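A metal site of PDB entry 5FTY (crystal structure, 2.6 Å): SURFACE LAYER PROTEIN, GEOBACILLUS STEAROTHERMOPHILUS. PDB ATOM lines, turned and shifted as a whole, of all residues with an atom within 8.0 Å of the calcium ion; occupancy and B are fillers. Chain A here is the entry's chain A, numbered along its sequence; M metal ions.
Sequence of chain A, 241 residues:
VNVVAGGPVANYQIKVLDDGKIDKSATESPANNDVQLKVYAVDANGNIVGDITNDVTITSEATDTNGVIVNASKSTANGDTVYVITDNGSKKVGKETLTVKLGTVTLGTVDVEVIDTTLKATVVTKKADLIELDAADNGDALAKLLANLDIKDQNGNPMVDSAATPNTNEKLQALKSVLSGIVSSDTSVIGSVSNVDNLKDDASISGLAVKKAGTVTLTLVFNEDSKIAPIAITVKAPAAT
The calcium ion is bound by O of Val 68 (2.4 Å), OE2 of Glu 61 (2.4 Å), OD1 of Asn 66 (2.6 Å), OE2 of Glu 96 (2.7 Å), OE1 of Glu 96 (2.7 Å) and OD1 of Asp 64 (2.8 Å). The calcium ion has six donor atoms within binding distance.
Of the 15 residues printed, 5 come within 4 Å of the calcium ion.
OD2 of Asp 64 lies within hydrogen-bond range of N of Gly 67. O of Lys 95 sits at hydrogen-bond distance from ND2 of Asn 66. OE1 of Glu 61 is in hydrogen-bond range of OG1 of Thr 65 (2.9 Å).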
ATOM      1  N   SER A  60      -2.448  -2.191 -20.613  1.00  0.00           N
ATOM      2  CA  SER A  60      -3.860  -2.554 -20.562  1.00  0.00           C
ATOM      3  C   SER A  60      -4.280  -3.080 -21.926  1.00  0.00           C
ATOM      4  O   SER A  60      -3.440  -3.306 -22.795  1.00  0.00           O
ATOM      5  CB  SER A  60      -4.721  -1.357 -20.146  1.00  0.00           C
ATOM      6  OG  SER A  60      -4.487  -0.239 -20.977  1.00  0.00           O
ATOM      7  N   GLU A  61      -5.587  -3.278 -22.108  1.00  0.00           N
ATOM      8  CA  GLU A  61      -6.128  -3.776 -23.374  1.00  0.00           C
ATOM      9  C   GLU A  61      -5.766  -2.865 -24.534  1.00  0.00           C
ATOM     10  O   GLU A  61      -5.736  -1.642 -24.399  1.00  0.00           O
ATOM     11  CB  GLU A  61      -7.652  -3.930 -23.268  1.00  0.00           C
ATOM     12  CG  GLU A  61      -8.359  -2.687 -22.784  1.00  0.00           C
ATOM     13  CD  GLU A  61      -9.824  -2.925 -22.475  1.00  0.00           C
ATOM     14  OE1 GLU A  61     -10.250  -4.095 -22.529  1.00  0.00           O
ATOM     15  OE2 GLU A  61     -10.548  -1.951 -22.189  1.00  0.00           O
ATOM     16  N   ALA A  62      -5.462  -3.470 -25.682  1.00  0.00           N
ATOM     17  CA  ALA A  62      -5.040  -2.715 -26.860  1.00  0.00           C
ATOM     18  C   ALA A  62      -6.199  -1.912 -27.449  1.00  0.00           C
ATOM     19  O   ALA A  62      -6.001  -0.848 -28.023  1.00  0.00           O
ATOM     20  CB  ALA A  62      -4.449  -3.650 -27.909  1.00  0.00           C
ATOM     21  N   THR A  63      -7.409  -2.435 -27.284  1.00  0.00           N
ATOM     22  CA  THR A  63      -8.610  -1.756 -27.747  1.00  0.00           C
ATOM     23  C   THR A  63      -9.598  -1.597 -26.589  1.00  0.00           C
ATOM     24  O   THR A  63      -9.932  -2.571 -25.924  1.00  0.00           O
ATOM     25  CB  THR A  63      -9.293  -2.517 -28.897  1.00  0.00           C
ATOM     26  OG1 THR A  63      -9.796  -3.770 -28.414  1.00  0.00           O
ATOM     27  CG2 THR A  63      -8.309  -2.787 -30.032  1.00  0.00           C
ATOM     28  N   ASP A  64     -10.064  -0.367 -26.379  1.00  0.00           N
ATOM     29  CA  ASP A  64     -10.956  -0.060 -25.265  1.00  0.00           C
ATOM     30  C   ASP A  64     -12.269  -0.832 -25.353  1.00  0.00           C
ATOM     31  O   ASP A  64     -12.860  -0.950 -26.422  1.00  0.00           O
ATOM     32  CB  ASP A  64     -11.241   1.444 -25.216  1.00  0.00           C
ATOM     33  CG  ASP A  64     -12.140   1.839 -24.064  1.00  0.00           C
ATOM     34  OD1 ASP A  64     -11.816   1.466 -22.911  1.00  0.00           O
ATOM     35  OD2 ASP A  64     -13.157   2.517 -24.311  1.00  0.00           O
ATOM     36  N   THR A  65     -12.719  -1.371 -24.219  1.00  0.00           N
ATOM     37  CA  THR A  65     -13.947  -2.149 -24.178  1.00  0.00           C
ATOM     38  C   THR A  65     -14.896  -1.696 -23.070  1.00  0.00           C
ATOM     39  O   THR A  65     -16.039  -2.156 -23.002  1.00  0.00           O
ATOM     40  CB  THR A  65     -13.667  -3.649 -23.972  1.00  0.00           C
ATOM     41  OG1 THR A  65     -13.155  -3.871 -22.648  1.00  0.00           O
ATOM     42  CG2 THR A  65     -12.661  -4.177 -24.988  1.00  0.00           C
ATOM     43  N   ASN A  66     -14.416  -0.819 -22.199  1.00  0.00           N
ATOM     44  CA  ASN A  66     -15.205  -0.427 -21.036  1.00  0.00           C
ATOM     45  C   ASN A  66     -15.275   1.086 -20.820  1.00  0.00           C
ATOM     46  O   ASN A  66     -15.907   1.547 -19.865  1.00  0.00           O
ATOM     47  CB  ASN A  66     -14.646  -1.095 -19.780  1.00  0.00           C
ATOM     48  CG  ASN A  66     -13.195  -0.781 -19.543  1.00  0.00           C
ATOM     49  OD1 ASN A  66     -12.458  -0.455 -20.480  1.00  0.00           O
ATOM     50  ND2 ASN A  66     -12.757  -0.856 -18.293  1.00  0.00           N
ATOM     51  N   GLY A  67     -14.647   1.847 -21.702  1.00  0.00           N
ATOM     52  CA  GLY A  67     -14.649   3.295 -21.588  1.00  0.00           C
ATOM     53  C   GLY A  67     -13.669   3.817 -20.560  1.00  0.00           C
ATOM     54  O   GLY A  67     -13.576   5.023 -20.334  1.00  0.00           O
ATOM     55  N   VAL A  68     -12.926   2.914 -19.930  1.00  0.00           N
ATOM     56  CA  VAL A  68     -11.883   3.288 -18.983  1.00  0.00           C
ATOM     57  C   VAL A  68     -10.518   3.196 -19.653  1.00  0.00           C
ATOM     58  O   VAL A  68     -10.005   2.100 -19.885  1.00  0.00           O
ATOM     59  CB  VAL A  68     -11.904   2.397 -17.728  1.00  0.00           C
ATOM     60  CG1 VAL A  68     -10.727   2.721 -16.819  1.00  0.00           C
ATOM     61  CG2 VAL A  68     -13.224   2.540 -16.985  1.00  0.00           C
ATOM     62  N   ILE A  69      -9.930   4.340 -19.973  1.00  0.00           N
ATOM     63  CA  ILE A  69      -8.639   4.380 -20.658  1.00  0.00           C
ATOM     64  C   ILE A  69      -7.562   5.038 -19.788  1.00  0.00           C
ATOM     65  O   ILE A  69      -7.684   6.202 -19.417  1.00  0.00           O
ATOM     66  CB  ILE A  69      -8.735   5.160 -21.993  1.00  0.00           C
ATOM     67  CG1 ILE A  69     -10.076   4.888 -22.683  1.00  0.00           C
ATOM     68  CG2 ILE A  69      -7.558   4.798 -22.892  1.00  0.00           C
ATOM     69  CD1 ILE A  69     -10.294   5.708 -23.940  1.00  0.00           C
ATOM     70  N   VAL A  70      -6.519   4.275 -19.475  1.00  0.00           N
ATOM     71  CA  VAL A  70      -5.430   4.776 -18.620  1.00  0.00           C
ATOM     72  C   VAL A  70      -4.074   4.759 -19.326  1.00  0.00           C
ATOM     73  O   VAL A  70      -3.937   4.219 -20.424  1.00  0.00           O
ATOM     74  CB  VAL A  70      -5.332   3.973 -17.305  1.00  0.00           C
ATOM     75  CG1 VAL A  70      -6.598   4.156 -16.465  1.00  0.00           C
ATOM     76  CG2 VAL A  70      -5.079   2.501 -17.594  1.00  0.00           C
ATOM     77  N   SER A  90     -10.657   8.705 -20.335  1.00  0.00           N
ATOM     78  CA  SER A  90     -11.717   7.745 -20.023  1.00  0.00           C
ATOM     79  C   SER A  90     -13.074   8.446 -19.951  1.00  0.00           C
ATOM     80  O   SER A  90     -13.202   9.510 -19.366  1.00  0.00           O
ATOM     81  CB  SER A  90     -11.415   7.033 -18.707  1.00  0.00           C
ATOM     82  OG  SER A  90     -10.931   7.948 -17.736  1.00  0.00           O
ATOM     83  N   LYS A  95     -13.301  -0.541 -13.369  1.00  0.00           N
ATOM     84  CA  LYS A  95     -12.054  -1.268 -13.258  1.00  0.00           C
ATOM     85  C   LYS A  95     -11.340  -1.411 -14.605  1.00  0.00           C
ATOM     86  O   LYS A  95     -11.968  -1.598 -15.642  1.00  0.00           O
ATOM     87  CB  LYS A  95     -12.302  -2.660 -12.671  1.00  0.00           C
ATOM     88  CG  LYS A  95     -12.954  -2.654 -11.291  1.00  0.00           C
ATOM     89  CD  LYS A  95     -12.058  -2.019 -10.257  1.00  0.00           C
ATOM     90  CE  LYS A  95     -12.508  -2.381  -8.845  1.00  0.00           C
ATOM     91  NZ  LYS A  95     -12.481  -3.859  -8.632  1.00  0.00           N
ATOM     92  N   GLU A  96     -10.015  -1.313 -14.571  1.00  0.00           N
ATOM     93  CA  GLU A  96      -9.194  -1.529 -15.754  1.00  0.00           C
ATOM     94  C   GLU A  96      -8.055  -2.485 -15.416  1.00  0.00           C
ATOM     95  O   GLU A  96      -7.194  -2.180 -14.602  1.00  0.00           O
ATOM     96  CB  GLU A  96      -8.622  -0.206 -16.266  1.00  0.00           C
ATOM     97  CG  GLU A  96      -7.792  -0.344 -17.533  1.00  0.00           C
ATOM     98  CD  GLU A  96      -8.631  -0.593 -18.773  1.00  0.00           C
ATOM     99  OE1 GLU A  96      -9.872  -0.506 -18.685  1.00  0.00           O
ATOM    100  OE2 GLU A  96      -8.040  -0.875 -19.842  1.00  0.00           O
ATOM    101  N   THR A  97      -8.067  -3.658 -16.045  1.00  0.00           N
ATOM    102  CA  THR A  97      -7.063  -4.669 -15.786  1.00  0.00           C
ATOM    103  C   THR A  97      -5.721  -4.300 -16.391  1.00  0.00           C
ATOM    104  O   THR A  97      -5.612  -4.077 -17.595  1.00  0.00           O
ATOM    105  CB  THR A  97      -7.494  -6.052 -16.335  1.00  0.00           C
ATOM    106  OG1 THR A  97      -8.741  -6.440 -15.727  1.00  0.00           O
ATOM    107  CG2 THR A  97      -6.445  -7.100 -16.028  1.00  0.00           C
HETATM  108 CA    CA M   1     -10.028   0.169 -21.262  1.00  0.00          CA
